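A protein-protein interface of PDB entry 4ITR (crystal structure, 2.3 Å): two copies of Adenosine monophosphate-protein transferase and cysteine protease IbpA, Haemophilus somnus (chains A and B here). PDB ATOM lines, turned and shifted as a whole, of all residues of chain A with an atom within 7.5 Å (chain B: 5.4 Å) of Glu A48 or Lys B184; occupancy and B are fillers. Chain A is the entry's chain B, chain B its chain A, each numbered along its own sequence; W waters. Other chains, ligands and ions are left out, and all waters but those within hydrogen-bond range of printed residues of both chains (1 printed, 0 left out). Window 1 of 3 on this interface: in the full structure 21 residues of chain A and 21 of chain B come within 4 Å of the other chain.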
ATOM      1  N   PHE A  42      14.934   9.643  28.245  1.00  0.00           N
ATOM      2  CA  PHE A  42      14.437   8.689  27.263  1.00  0.00           C
ATOM      3  C   PHE A  42      12.937   8.856  27.073  1.00  0.00           C
ATOM      4  O   PHE A  42      12.439   8.833  25.948  1.00  0.00           O
ATOM      5  CB  PHE A  42      14.755   7.255  27.693  1.00  0.00           C
ATOM      6  CG  PHE A  42      14.004   6.208  26.916  1.00  0.00           C
ATOM      7  CD1 PHE A  42      14.380   5.882  25.619  1.00  0.00           C
ATOM      8  CD2 PHE A  42      12.921   5.551  27.482  1.00  0.00           C
ATOM      9  CE1 PHE A  42      13.687   4.920  24.902  1.00  0.00           C
ATOM     10  CE2 PHE A  42      12.226   4.589  26.773  1.00  0.00           C
ATOM     11  CZ  PHE A  42      12.608   4.274  25.480  1.00  0.00           C
ATOM     12  N   LEU A  43      12.220   9.021  28.182  1.00  0.00           N
ATOM     13  CA  LEU A  43      10.770   9.201  28.133  1.00  0.00           C
ATOM     14  C   LEU A  43      10.387  10.495  27.421  1.00  0.00           C
ATOM     15  O   LEU A  43       9.470  10.501  26.595  1.00  0.00           O
ATOM     16  CB  LEU A  43      10.166   9.159  29.539  1.00  0.00           C
ATOM     17  CG  LEU A  43      10.153   7.795  30.234  1.00  0.00           C
ATOM     18  CD1 LEU A  43       9.523   7.891  31.612  1.00  0.00           C
ATOM     19  CD2 LEU A  43       9.420   6.772  29.389  1.00  0.00           C
ATOM     20  N   ASP A  44      11.087  11.584  27.737  1.00  0.00           N
ATOM     21  CA  ASP A  44      10.852  12.864  27.072  1.00  0.00           C
ATOM     22  C   ASP A  44      11.075  12.741  25.573  1.00  0.00           C
ATOM     23  O   ASP A  44      10.323  13.300  24.775  1.00  0.00           O
ATOM     24  CB  ASP A  44      11.771  13.948  27.640  1.00  0.00           C
ATOM     25  CG  ASP A  44      11.171  14.659  28.834  1.00  0.00           C
ATOM     26  OD1 ASP A  44       9.996  14.388  29.164  1.00  0.00           O
ATOM     27  OD2 ASP A  44      11.874  15.501  29.433  1.00  0.00           O
ATOM     28  N   GLU A  45      12.119  12.009  25.198  1.00  0.00           N
ATOM     29  CA  GLU A  45      12.423  11.766  23.792  1.00  0.00           C
ATOM     30  C   GLU A  45      11.241  11.087  23.111  1.00  0.00           C
ATOM     31  O   GLU A  45      10.811  11.496  22.033  1.00  0.00           O
ATOM     32  CB  GLU A  45      13.666  10.884  23.673  1.00  0.00           C
ATOM     33  CG  GLU A  45      14.119  10.636  22.245  1.00  0.00           C
ATOM     34  CD  GLU A  45      15.213   9.594  22.158  1.00  0.00           C
ATOM     35  OE1 GLU A  45      14.984   8.449  22.604  1.00  0.00           O
ATOM     36  OE2 GLU A  45      16.304   9.918  21.644  1.00  0.00           O
ATOM     37  N   ALA A  46      10.719  10.054  23.761  1.00  0.00           N
ATOM     38  CA  ALA A  46       9.578   9.308  23.245  1.00  0.00           C
ATOM     39  C   ALA A  46       8.349  10.201  23.123  1.00  0.00           C
ATOM     40  O   ALA A  46       7.627  10.146  22.122  1.00  0.00           O
ATOM     41  CB  ALA A  46       9.286   8.122  24.145  1.00  0.00           C
ATOM     42  N   ARG A  47       8.114  11.014  24.149  1.00  0.00           N
ATOM     43  CA  ARG A  47       6.974  11.925  24.168  1.00  0.00           C
ATOM     44  C   ARG A  47       7.035  12.919  23.011  1.00  0.00           C
ATOM     45  O   ARG A  47       6.017  13.218  22.388  1.00  0.00           O
ATOM     46  CB  ARG A  47       6.910  12.681  25.500  1.00  0.00           C
ATOM     47  CG  ARG A  47       6.633  11.814  26.717  1.00  0.00           C
ATOM     48  CD  ARG A  47       6.794  12.604  28.011  1.00  0.00           C
ATOM     49  NE  ARG A  47       6.615  11.765  29.196  1.00  0.00           N
ATOM     50  CZ  ARG A  47       7.486  11.682  30.198  1.00  0.00           C
ATOM     51  NH1 ARG A  47       8.608  12.389  30.169  1.00  0.00           N
ATOM     52  NH2 ARG A  47       7.235  10.891  31.230  1.00  0.00           N
ATOM     53  N   GLU A  48       8.233  13.420  22.722  1.00  0.00           N
ATOM     54  CA  GLU A  48       8.408  14.391  21.644  1.00  0.00           C
ATOM     55  C   GLU A  48       8.225  13.746  20.272  1.00  0.00           C
ATOM     56  O   GLU A  48       7.557  14.306  19.403  1.00  0.00           O
ATOM     57  CB  GLU A  48       9.783  15.061  21.738  1.00  0.00           C
ATOM     58  CG  GLU A  48       9.955  16.242  20.790  1.00  0.00           C
ATOM     59  CD  GLU A  48      11.282  16.956  20.974  1.00  0.00           C
ATOM     60  OE1 GLU A  48      12.059  16.552  21.866  1.00  0.00           O
ATOM     61  OE2 GLU A  48      11.546  17.922  20.226  1.00  0.00           O
ATOM     62  N   ILE A  49       8.824  12.571  20.089  1.00  0.00           N
ATOM     63  CA  ILE A  49       8.686  11.805  18.853  1.00  0.00           C
ATOM     64  C   ILE A  49       7.218  11.529  18.542  1.00  0.00           C
ATOM     65  O   ILE A  49       6.759  11.749  17.420  1.00  0.00           O
ATOM     66  CB  ILE A  49       9.439  10.459  18.942  1.00  0.00           C
ATOM     67  CG1 ILE A  49      10.949  10.683  18.871  1.00  0.00           C
ATOM     68  CG2 ILE A  49       9.001   9.517  17.825  1.00  0.00           C
ATOM     69  CD1 ILE A  49      11.767   9.469  19.265  1.00  0.00           C
ATOM     70  N   SER A  50       6.487  11.056  19.547  1.00  0.00           N
ATOM     71  CA  SER A  50       5.085  10.686  19.386  1.00  0.00           C
ATOM     72  C   SER A  50       4.189  11.873  19.032  1.00  0.00           C
ATOM     73  O   SER A  50       3.286  11.745  18.204  1.00  0.00           O
ATOM     74  CB  SER A  50       4.576  10.012  20.660  1.00  0.00           C
ATOM     75  OG  SER A  50       5.356   8.877  20.980  1.00  0.00           O
ATOM     76  N   LYS A  51       4.443  13.019  19.657  1.00  0.00           N
ATOM     77  CA  LYS A  51       3.611  14.208  19.471  1.00  0.00           C
ATOM     78  C   LYS A  51       3.737  14.837  18.086  1.00  0.00           C
ATOM     79  O   LYS A  51       2.850  15.576  17.655  1.00  0.00           O
ATOM     80  CB  LYS A  51       3.932  15.263  20.536  1.00  0.00           C
ATOM     81  CG  LYS A  51       3.207  15.068  21.867  1.00  0.00           C
ATOM     82  CD  LYS A  51       3.569  16.166  22.865  1.00  0.00           C
ATOM     83  CE  LYS A  51       2.772  16.026  24.158  1.00  0.00           C
ATOM     84  NZ  LYS A  51       3.182  17.005  25.211  1.00  0.00           N
ATOM     85  N   LYS A  52       4.839  14.551  17.396  1.00  0.00           N
ATOM     86  CA  LYS A  52       5.113  15.160  16.094  1.00  0.00           C
ATOM     87  C   LYS A  52       4.038  14.853  15.050  1.00  0.00           C
ATOM     88  O   LYS A  52       3.726  15.695  14.209  1.00  0.00           O
ATOM     89  CB  LYS A  52       6.494  14.738  15.572  1.00  0.00           C
ATOM     90  CG  LYS A  52       7.663  15.336  16.342  1.00  0.00           C
ATOM     91  CD  LYS A  52       8.992  15.137  15.614  1.00  0.00           C
ATOM     92  CE  LYS A  52       9.293  13.667  15.379  1.00  0.00           C
ATOM     93  NZ  LYS A  52      10.637  13.436  14.772  1.00  0.00           N
ATOM     94  N   SER A  53       3.470  13.651  15.115  1.00  0.00           N
ATOM     95  CA  SER A  53       2.466  13.226  14.141  1.00  0.00           C
ATOM     96  C   SER A  53       1.034  13.492  14.601  1.00  0.00           C
ATOM     97  O   SER A  53       0.086  13.293  13.842  1.00  0.00           O
ATOM     98  CB  SER A  53       2.630  11.740  13.812  1.00  0.00           C
ATOM     99  OG  SER A  53       3.820  11.502  13.088  1.00  0.00           O
ATOM    100  N   LEU A  72       1.894   7.579  24.847  1.00  0.00           N
ATOM    101  CA  LEU A  72       3.038   8.247  24.236  1.00  0.00           C
ATOM    102  C   LEU A  72       4.319   7.415  24.310  1.00  0.00           C
ATOM    103  O   LEU A  72       5.119   7.404  23.371  1.00  0.00           O
ATOM    104  CB  LEU A  72       3.259   9.601  24.913  1.00  0.00           C
ATOM    105  CG  LEU A  72       2.869  10.865  24.150  1.00  0.00           C
ATOM    106  CD1 LEU A  72       1.747  10.583  23.179  1.00  0.00           C
ATOM    107  CD2 LEU A  72       2.478  11.984  25.107  1.00  0.00           C
ATOM    108  N   THR A  73       4.502   6.715  25.426  1.00  0.00           N
ATOM    109  CA  THR A  73       5.764   6.035  25.714  1.00  0.00           C
ATOM    110  C   THR A  73       5.724   4.519  25.519  1.00  0.00           C
ATOM    111  O   THR A  73       6.767   3.864  25.538  1.00  0.00           O
ATOM    112  CB  THR A  73       6.227   6.336  27.153  1.00  0.00           C
ATOM    113  OG1 THR A  73       5.223   5.907  28.080  1.00  0.00           O
ATOM    114  CG2 THR A  73       6.467   7.826  27.332  1.00  0.00           C
ATOM    115  N   LEU B 180       6.429  17.258  28.419  1.00  0.00           N
ATOM    116  CA  LEU B 180       7.849  16.959  28.572  1.00  0.00           C
ATOM    117  C   LEU B 180       8.327  17.516  29.903  1.00  0.00           C
ATOM    118  O   LEU B 180       7.936  18.617  30.291  1.00  0.00           O
ATOM    119  CB  LEU B 180       8.657  17.602  27.444  1.00  0.00           C
ATOM    120  CG  LEU B 180       8.172  17.409  26.008  1.00  0.00           C
ATOM    121  CD1 LEU B 180       9.038  18.197  25.043  1.00  0.00           C
ATOM    122  CD2 LEU B 180       8.190  15.948  25.645  1.00  0.00           C
ATOM    123  N   TYR B 182      11.801  17.937  30.833  1.00  0.00           N
ATOM    124  CA  TYR B 182      12.860  18.862  30.451  1.00  0.00           C
ATOM    125  C   TYR B 182      12.430  19.691  29.250  1.00  0.00           C
ATOM    126  O   TYR B 182      11.591  19.259  28.455  1.00  0.00           O
ATOM    127  CB  TYR B 182      14.139  18.088  30.123  1.00  0.00           C
ATOM    128  CG  TYR B 182      14.809  17.478  31.331  1.00  0.00           C
ATOM    129  CD1 TYR B 182      15.738  18.199  32.066  1.00  0.00           C
ATOM    130  CD2 TYR B 182      14.513  16.183  31.737  1.00  0.00           C
ATOM    131  CE1 TYR B 182      16.353  17.652  33.170  1.00  0.00           C
ATOM    132  CE2 TYR B 182      15.122  15.628  32.841  1.00  0.00           C
ATOM    133  CZ  TYR B 182      16.040  16.368  33.553  1.00  0.00           C
ATOM    134  OH  TYR B 182      16.653  15.818  34.654  1.00  0.00           O
ATOM    135  N   LYS B 183      12.995  20.889  29.126  1.00  0.00           N
ATOM    136  CA  LYS B 183      12.751  21.720  27.952  1.00  0.00           C
ATOM    137  C   LYS B 183      13.419  21.078  26.742  1.00  0.00           C
ATOM    138  O   LYS B 183      14.481  20.465  26.864  1.00  0.00           O
ATOM    139  CB  LYS B 183      13.269  23.145  28.171  1.00  0.00           C
ATOM    140  CG  LYS B 183      14.767  23.245  28.412  1.00  0.00           C
ATOM    141  CD  LYS B 183      15.158  24.650  28.846  1.00  0.00           C
ATOM    142  CE  LYS B 183      16.670  24.800  28.957  1.00  0.00           C
ATOM    143  NZ  LYS B 183      17.041  26.034  29.710  1.00  0.00           N
ATOM    144  N   LYS B 184      12.788  21.201  25.579  1.00  0.00           N
ATOM    145  CA  LYS B 184      13.288  20.542  24.376  1.00  0.00           C
ATOM    146  C   LYS B 184      14.046  21.499  23.466  1.00  0.00           C
ATOM    147  O   LYS B 184      14.600  21.089  22.442  1.00  0.00           O
ATOM    148  CB  LYS B 184      12.133  19.900  23.606  1.00  0.00           C
ATOM    149  CG  LYS B 184      11.098  20.890  23.095  1.00  0.00           C
ATOM    150  CD  LYS B 184      10.081  20.197  22.199  1.00  0.00           C
ATOM    151  CE  LYS B 184       9.077  21.186  21.630  1.00  0.00           C
ATOM    152  NZ  LYS B 184       8.163  20.533  20.653  1.00  0.00           N
ATOM    153  N   GLU B 185      14.078  22.771  23.844  1.00  0.00           N
ATOM    154  CA  GLU B 185      14.698  23.796  23.013  1.00  0.00           C
ATOM    155  C   GLU B 185      15.170  24.960  23.868  1.00  0.00           C
ATOM    156  O   GLU B 185      14.819  25.059  25.044  1.00  0.00           O
ATOM    157  CB  GLU B 185      13.695  24.298  21.971  1.00  0.00           C
ATOM    158  CG  GLU B 185      12.401  24.831  22.574  1.00  0.00           C
ATOM    159  CD  GLU B 185      11.340  25.087  21.530  1.00  0.00           C
ATOM    160  OE1 GLU B 185      10.151  25.174  21.901  1.00  0.00           O
ATOM    161  OE2 GLU B 185      11.695  25.204  20.339  1.00  0.00           O
ATOM    162  N   ASN B 186      15.971  25.842  23.277  1.00  0.00           N
ATOM    163  CA  ASN B 186      16.344  27.075  23.956  1.00  0.00           C
ATOM    164  C   ASN B 186      15.108  27.928  24.205  1.00  0.00           C
ATOM    165  O   ASN B 186      14.402  28.302  23.268  1.00  0.00           O
ATOM    166  CB  ASN B 186      17.383  27.857  23.151  1.00  0.00           C
ATOM    167  CG  ASN B 186      18.776  27.261  23.262  1.00  0.00           C
ATOM    168  OD1 ASN B 186      19.374  27.254  24.337  1.00  0.00           O
ATOM    169  ND2 ASN B 186      19.306  26.774  22.145  1.00  0.00           N
ATOM    170  N   PRO B 197      19.324  23.062  26.511  1.00  0.00           N
ATOM    171  CA  PRO B 197      18.797  21.859  27.169  1.00  0.00           C
ATOM    172  C   PRO B 197      19.875  20.875  27.636  1.00  0.00           C
ATOM    173  O   PRO B 197      19.821  20.431  28.784  1.00  0.00           O
ATOM    174  CB  PRO B 197      17.932  21.224  26.079  1.00  0.00           C
ATOM    175  CG  PRO B 197      17.458  22.383  25.270  1.00  0.00           C
ATOM    176  CD  PRO B 197      18.594  23.372  25.266  1.00  0.00           C
HETATM  177  O   HOH W   1      12.485  17.491  26.741  1.00  0.00           O
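Water W1 lies within hydrogen-bond range of the backbone carbonyl oxygen (O) of Tyr B182 and the side-chain carboxylate (OD2) of Asp A44.
Printed residues of chain A that touch a printed residue of chain B: Asp A44, Arg A47 and Glu A48.
Among the printed residues, no Asp or Glu carboxylate lies within 4 Å of a Lys or Arg side-chain nitrogen of the other chain.
The side-chain carboxylate of Asp A44 is in hydrogen-bond range of the backbone NH of Tyr B182, 2.8 Å away.
The guanidinium group (NH1) of Arg A47 is in salt-bridge range of the side-chain carboxylate (OD1) of Asp A44.
Of the printed residues of chain B, Asp A44 touches Leu B180 (3.4 Å) and Tyr B182 (2.8 Å).
Printed residues of chain B within 4 Å of Arg A47: Leu B180.
Of the printed residues of chain B, Glu A48 touches Leu B180 (3.9 Å) and Lys B184 (3.3 Å).
Of the printed residues of chain A, Leu B180 touches Asp A44, Arg A47 and Glu A48.
Lys B184 touches just one residue of chain A: Glu A48.
Glu B185 touches none of the printed residues of chain A.
The nearest printed residue of chain B that does not touch Glu A48 is Glu B185 (6.6 Å).
No position is printed for both chains.
Of the 5 pairs that touch across the chains among the printed residues, none has its exchanged pair printed and touching as well.
Asp A44 touches Leu B180 (OD1 to CA, 3.4 Å).
Leu B180 touches Arg A47 (CD2 to CB, 3.5 Å).
N of Glu A48 touches CD2 of Leu B180, at 3.9 Å.
Lys B184 touches Glu A48 (CD to OE2, 3.3 Å).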
